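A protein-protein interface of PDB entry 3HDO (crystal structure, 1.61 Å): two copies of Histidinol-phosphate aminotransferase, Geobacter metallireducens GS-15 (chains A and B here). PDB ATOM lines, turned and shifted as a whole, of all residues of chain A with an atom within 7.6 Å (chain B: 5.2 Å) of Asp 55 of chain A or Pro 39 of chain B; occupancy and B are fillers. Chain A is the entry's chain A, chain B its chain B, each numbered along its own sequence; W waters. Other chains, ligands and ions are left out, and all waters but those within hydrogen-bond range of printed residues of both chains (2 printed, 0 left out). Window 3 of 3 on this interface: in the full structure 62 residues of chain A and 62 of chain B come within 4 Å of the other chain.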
ATOM      1  N   GLU A  51     -21.166  11.913  -2.205  1.00  0.00           N
ATOM      2  CA  GLU A  51     -20.217  11.019  -2.860  1.00  0.00           C
ATOM      3  C   GLU A  51     -20.286   9.627  -2.240  1.00  0.00           C
ATOM      4  O   GLU A  51     -20.245   8.621  -2.949  1.00  0.00           O
ATOM      5  CB  GLU A  51     -18.797  11.588  -2.742  1.00  0.00           C
ATOM      6  CG  GLU A  51     -17.709  10.792  -3.460  1.00  0.00           C
ATOM      7  CD  GLU A  51     -17.891  10.731  -4.970  1.00  0.00           C
ATOM      8  OE1 GLU A  51     -18.449  11.682  -5.557  1.00  0.00           O
ATOM      9  OE2 GLU A  51     -17.455   9.731  -5.577  1.00  0.00           O
ATOM     10  N   LEU A  52     -20.411   9.568  -0.917  1.00  0.00           N
ATOM     11  CA  LEU A  52     -20.488   8.286  -0.230  1.00  0.00           C
ATOM     12  C   LEU A  52     -21.747   7.533  -0.644  1.00  0.00           C
ATOM     13  O   LEU A  52     -21.712   6.330  -0.889  1.00  0.00           O
ATOM     14  CB  LEU A  52     -20.491   8.489   1.289  1.00  0.00           C
ATOM     15  CG  LEU A  52     -20.622   7.215   2.132  1.00  0.00           C
ATOM     16  CD1 LEU A  52     -19.432   6.293   1.895  1.00  0.00           C
ATOM     17  CD2 LEU A  52     -20.712   7.596   3.598  1.00  0.00           C
ATOM     18  N   GLY A  53     -22.860   8.251  -0.727  1.00  0.00           N
ATOM     19  CA  GLY A  53     -24.108   7.618  -1.102  1.00  0.00           C
ATOM     20  C   GLY A  53     -24.659   6.750   0.014  1.00  0.00           C
ATOM     21  O   GLY A  53     -24.072   6.660   1.092  1.00  0.00           O
ATOM     22  N   PRO A  54     -25.793   6.081  -0.220  1.00  0.00           N
ATOM     23  CA  PRO A  54     -26.420   5.217   0.784  1.00  0.00           C
ATOM     24  C   PRO A  54     -25.682   3.914   1.085  1.00  0.00           C
ATOM     25  O   PRO A  54     -25.779   3.391   2.200  1.00  0.00           O
ATOM     26  CB  PRO A  54     -27.810   4.969   0.200  1.00  0.00           C
ATOM     27  CG  PRO A  54     -27.557   5.003  -1.274  1.00  0.00           C
ATOM     28  CD  PRO A  54     -26.645   6.198  -1.416  1.00  0.00           C
ATOM     29  N   ASP A  55     -24.938   3.401   0.106  1.00  0.00           N
ATOM     30  CA  ASP A  55     -24.222   2.137   0.278  1.00  0.00           C
ATOM     31  C   ASP A  55     -22.726   2.196  -0.016  1.00  0.00           C
ATOM     32  O   ASP A  55     -22.065   1.156  -0.061  1.00  0.00           O
ATOM     33  CB  ASP A  55     -24.852   1.060  -0.612  1.00  0.00           C
ATOM     34  CG  ASP A  55     -24.796   1.415  -2.089  1.00  0.00           C
ATOM     35  OD1 ASP A  55     -24.198   2.456  -2.437  1.00  0.00           O
ATOM     36  OD2 ASP A  55     -25.352   0.650  -2.905  1.00  0.00           O
ATOM     37  N   GLY A  56     -22.200   3.397  -0.227  1.00  0.00           N
ATOM     38  CA  GLY A  56     -20.781   3.542  -0.510  1.00  0.00           C
ATOM     39  C   GLY A  56     -20.321   2.903  -1.809  1.00  0.00           C
ATOM     40  O   GLY A  56     -19.125   2.702  -2.013  1.00  0.00           O
ATOM     41  N   ALA A  57     -21.258   2.597  -2.701  1.00  0.00           N
ATOM     42  CA  ALA A  57     -20.918   1.966  -3.972  1.00  0.00           C
ATOM     43  C   ALA A  57     -19.826   2.694  -4.755  1.00  0.00           C
ATOM     44  O   ALA A  57     -18.975   2.059  -5.381  1.00  0.00           O
ATOM     45  CB  ALA A  57     -22.168   1.832  -4.834  1.00  0.00           C
ATOM     46  N   ALA A  58     -19.848   4.023  -4.722  1.00  0.00           N
ATOM     47  CA  ALA A  58     -18.863   4.821  -5.446  1.00  0.00           C
ATOM     48  C   ALA A  58     -17.427   4.559  -5.008  1.00  0.00           C
ATOM     49  O   ALA A  58     -16.494   4.753  -5.788  1.00  0.00           O
ATOM     50  CB  ALA A  58     -19.181   6.302  -5.291  1.00  0.00           C
ATOM     51  N   LEU A  59     -17.248   4.117  -3.767  1.00  0.00           N
ATOM     52  CA  LEU A  59     -15.909   3.860  -3.249  1.00  0.00           C
ATOM     53  C   LEU A  59     -15.209   2.658  -3.879  1.00  0.00           C
ATOM     54  O   LEU A  59     -14.016   2.468  -3.683  1.00  0.00           O
ATOM     55  CB  LEU A  59     -15.947   3.710  -1.721  1.00  0.00           C
ATOM     56  CG  LEU A  59     -16.457   4.938  -0.955  1.00  0.00           C
ATOM     57  CD1 LEU A  59     -16.261   4.716   0.541  1.00  0.00           C
ATOM     58  CD2 LEU A  59     -15.700   6.190  -1.409  1.00  0.00           C
ATOM     59  N   ARG A  60     -15.933   1.851  -4.646  1.00  0.00           N
ATOM     60  CA  ARG A  60     -15.295   0.699  -5.282  1.00  0.00           C
ATOM     61  C   ARG A  60     -14.545   1.139  -6.537  1.00  0.00           C
ATOM     62  O   ARG A  60     -13.753   0.377  -7.100  1.00  0.00           O
ATOM     63  CB  ARG A  60     -16.335  -0.363  -5.647  1.00  0.00           C
ATOM     64  CG  ARG A  60     -17.158  -0.040  -6.880  1.00  0.00           C
ATOM     65  CD  ARG A  60     -18.265  -1.067  -7.065  1.00  0.00           C
ATOM     66  NE  ARG A  60     -18.909  -0.955  -8.369  1.00  0.00           N
ATOM     67  CZ  ARG A  60     -19.659   0.070  -8.755  1.00  0.00           C
ATOM     68  NH1 ARG A  60     -19.870   1.094  -7.938  1.00  0.00           N
ATOM     69  NH2 ARG A  60     -20.206   0.068  -9.963  1.00  0.00           N
ATOM     70  N   PRO B  37     -16.787  -5.505  -8.221  1.00  0.00           N
ATOM     71  CA  PRO B  37     -18.101  -5.167  -8.773  1.00  0.00           C
ATOM     72  C   PRO B  37     -19.139  -4.806  -7.716  1.00  0.00           C
ATOM     73  O   PRO B  37     -20.164  -4.210  -8.030  1.00  0.00           O
ATOM     74  CB  PRO B  37     -18.485  -6.428  -9.543  1.00  0.00           C
ATOM     75  CG  PRO B  37     -17.881  -7.513  -8.722  1.00  0.00           C
ATOM     76  CD  PRO B  37     -16.519  -6.950  -8.329  1.00  0.00           C
ATOM     77  N   TYR B  38     -18.855  -5.149  -6.465  1.00  0.00           N
ATOM     78  CA  TYR B  38     -19.794  -4.902  -5.373  1.00  0.00           C
ATOM     79  C   TYR B  38     -19.389  -3.751  -4.461  1.00  0.00           C
ATOM     80  O   TYR B  38     -18.216  -3.398  -4.372  1.00  0.00           O
ATOM     81  CB  TYR B  38     -19.940  -6.178  -4.543  1.00  0.00           C
ATOM     82  CG  TYR B  38     -20.154  -7.410  -5.390  1.00  0.00           C
ATOM     83  CD1 TYR B  38     -21.268  -7.519  -6.222  1.00  0.00           C
ATOM     84  CD2 TYR B  38     -19.222  -8.447  -5.396  1.00  0.00           C
ATOM     85  CE1 TYR B  38     -21.446  -8.628  -7.045  1.00  0.00           C
ATOM     86  CE2 TYR B  38     -19.392  -9.560  -6.213  1.00  0.00           C
ATOM     87  CZ  TYR B  38     -20.503  -9.641  -7.036  1.00  0.00           C
ATOM     88  OH  TYR B  38     -20.659 -10.731  -7.858  1.00  0.00           O
ATOM     89  N   PRO B  39     -20.366  -3.147  -3.769  1.00  0.00           N
ATOM     90  CA  PRO B  39     -20.059  -2.036  -2.865  1.00  0.00           C
ATOM     91  C   PRO B  39     -19.289  -2.559  -1.662  1.00  0.00           C
ATOM     92  O   PRO B  39     -19.251  -3.764  -1.416  1.00  0.00           O
ATOM     93  CB  PRO B  39     -21.442  -1.527  -2.443  1.00  0.00           C
ATOM     94  CG  PRO B  39     -22.356  -2.005  -3.527  1.00  0.00           C
ATOM     95  CD  PRO B  39     -21.817  -3.378  -3.842  1.00  0.00           C
ATOM     96  N   PRO B  40     -18.647  -1.662  -0.906  1.00  0.00           N
ATOM     97  CA  PRO B  40     -17.910  -2.133   0.267  1.00  0.00           C
ATOM     98  C   PRO B  40     -18.923  -2.587   1.316  1.00  0.00           C
ATOM     99  O   PRO B  40     -20.133  -2.419   1.140  1.00  0.00           O
ATOM    100  CB  PRO B  40     -17.127  -0.895   0.704  1.00  0.00           C
ATOM    101  CG  PRO B  40     -18.021   0.239   0.272  1.00  0.00           C
ATOM    102  CD  PRO B  40     -18.475  -0.213  -1.099  1.00  0.00           C
ATOM    103  N   SER B  41     -18.433  -3.165   2.402  1.00  0.00           N
ATOM    104  CA  SER B  41     -19.319  -3.622   3.462  1.00  0.00           C
ATOM    105  C   SER B  41     -20.225  -2.510   3.977  1.00  0.00           C
ATOM    106  O   SER B  41     -19.807  -1.357   4.086  1.00  0.00           O
ATOM    107  CB  SER B  41     -18.504  -4.153   4.636  1.00  0.00           C
ATOM    108  OG  SER B  41     -19.319  -4.281   5.791  1.00  0.00           O
ATOM    109  N   VAL B  45     -19.803   1.896   5.403  1.00  0.00           N
ATOM    110  CA  VAL B  45     -20.634   3.078   5.225  1.00  0.00           C
ATOM    111  C   VAL B  45     -21.011   3.642   6.595  1.00  0.00           C
ATOM    112  O   VAL B  45     -20.896   4.844   6.831  1.00  0.00           O
ATOM    113  CB  VAL B  45     -21.919   2.737   4.438  1.00  0.00           C
ATOM    114  CG1 VAL B  45     -22.764   3.984   4.245  1.00  0.00           C
ATOM    115  CG2 VAL B  45     -21.549   2.133   3.089  1.00  0.00           C
ATOM    116  N   SER B 217     -13.406  -3.554  -2.007  1.00  0.00           N
ATOM    117  CA  SER B 217     -14.200  -2.550  -2.710  1.00  0.00           C
ATOM    118  C   SER B 217     -13.931  -1.124  -2.237  1.00  0.00           C
ATOM    119  O   SER B 217     -14.857  -0.325  -2.125  1.00  0.00           O
ATOM    120  CB  SER B 217     -15.695  -2.856  -2.541  1.00  0.00           C
ATOM    121  OG  SER B 217     -16.006  -4.162  -2.997  1.00  0.00           O
ATOM    122  N   TYR B 262     -18.473 -10.627   4.823  1.00  0.00           N
ATOM    123  CA  TYR B 262     -18.795  -9.921   3.588  1.00  0.00           C
ATOM    124  C   TYR B 262     -17.677 -10.129   2.571  1.00  0.00           C
ATOM    125  O   TYR B 262     -17.940 -10.413   1.400  1.00  0.00           O
ATOM    126  CB  TYR B 262     -18.978  -8.430   3.862  1.00  0.00           C
ATOM    127  CG  TYR B 262     -19.500  -7.665   2.670  1.00  0.00           C
ATOM    128  CD1 TYR B 262     -20.814  -7.820   2.242  1.00  0.00           C
ATOM    129  CD2 TYR B 262     -18.673  -6.804   1.955  1.00  0.00           C
ATOM    130  CE1 TYR B 262     -21.297  -7.136   1.129  1.00  0.00           C
ATOM    131  CE2 TYR B 262     -19.144  -6.115   0.841  1.00  0.00           C
ATOM    132  CZ  TYR B 262     -20.456  -6.284   0.435  1.00  0.00           C
ATOM    133  OH  TYR B 262     -20.929  -5.591  -0.657  1.00  0.00           O
ATOM    134  N   CYS B 266     -18.133 -11.804  -1.113  1.00  0.00           N
ATOM    135  CA  CYS B 266     -17.781 -11.097  -2.339  1.00  0.00           C
ATOM    136  C   CYS B 266     -16.746 -11.873  -3.137  1.00  0.00           C
ATOM    137  O   CYS B 266     -16.851 -11.974  -4.358  1.00  0.00           O
ATOM    138  CB  CYS B 266     -17.237  -9.705  -2.019  1.00  0.00           C
ATOM    139  SG  CYS B 266     -18.503  -8.537  -1.519  1.00  0.00           S
HETATM  140  O   HOH W   1     -22.657  -1.270   1.309  1.00  0.00           O
HETATM  141  O   HOH W   2     -20.526  -3.052 -10.662  1.00  0.00           O
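Of chain B, only Pro 39 (3.6 Å), Pro 40 (3.98 Å) and Val 45 (3.3 Å) come within 4 Å of Asp 55 of chain A.
Of the printed residues of chain B, Gly 56 of chain A touches Pro 40 and Val 45.
Of the printed residues of chain B, Arg 60 of chain A touches Pro 37, Tyr 38 and Ser 217.
Of chain A, only Asp 55 and Ala 57 come within 4 Å of Pro 39 of chain B.
Of the printed residues of chain A, Pro 40 of chain B touches Asp 55 (3.98 Å) and Gly 56 (3.1 Å).
Printed residues of chain A within 4 Å of Val 45 of chain B: Pro 54, Asp 55 and Gly 56.
Of the printed residues of chain A, Ser 217 of chain B touches Leu 59 (3.3 Å) and Arg 60 (3.3 Å).
The nearest printed residue of chain B that does not touch Asp 55 of chain A is Ser 41 of chain B (5.3 Å).
CG1 of Val 45 of chain B touches O of Pro 54 of chain A (3.7 Å).
O of Asp 55 of chain A touches CB of Pro 39 of chain B, 3.6 Å away.
Asp 55 of chain A touches Pro 40 of chain B.
CG2 of Val 45 of chain B touches C of Asp 55 of chain A, 3.3 Å away.
O of Gly 56 of chain A touches CD of Pro 40 of chain B, at 3.1 Å.
N of Gly 56 of chain A touches CG2 of Val 45 of chain B, 3.6 Å away.
CB of Pro 39 of chain B touches CA of Ala 57 of chain A (3.8 Å).
Arg 60 of chain A touches Pro 37 of chain B (NE to O, 3.5 Å).
Arg 60 of chain A touches Tyr 38 of chain B (CD to O, 3.6 Å).
Of the 9 printed residues of chain B, 6 touch a printed residue of chain A.
Hydrophobic or aromatic side chains of chain B within 4 Å of the printed part of chain A: Pro 39, Pro 40 and Val 45.
Of the 10 printed residues of chain A, 6 touch a printed residue of chain B.
Printed residues of chain A that touch a printed residue of chain B: Pro 54, Asp 55, Gly 56, Ala 57, Leu 59 and Arg 60.
Water W1 bridges O of Pro 40 of chain B (2.8 Å) and O of Asp 55 of chain A (2.8 Å).
Water W2 lies within hydrogen-bond range of O of Pro 37 of chain B (2.9 Å) and NH2 of Arg 60 of chain A (3.2 Å).
N of Ala 57 of chain A lies within hydrogen-bond range of OD1 of Asp 55 of chain A (3.0 Å).
The backbone carbonyl oxygen (O) of Ala 57 of chain A lies within hydrogen-bond range of the guanidinium group (NH1) of Arg 60 of chain A, 2.9 Å away.
O of Tyr 38 of chain B sits at hydrogen-bond distance from OG of Ser 217 of chain B.
The backbone carbonyl oxygen of Pro 39 of chain B lies within hydrogen-bond range of the side-chain hydroxyl of Tyr 262 of chain B (2.6 Å).
No position is printed for both chains.
O of Ser 217 of chain B sits close to N of Arg 60 of chain A (3.5 Å).
The backbone carbonyl oxygen (O) of Leu 59 of chain A sits close to the backbone carbonyl oxygen (O) of Ser 217 of chain B, 3.3 Å away.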
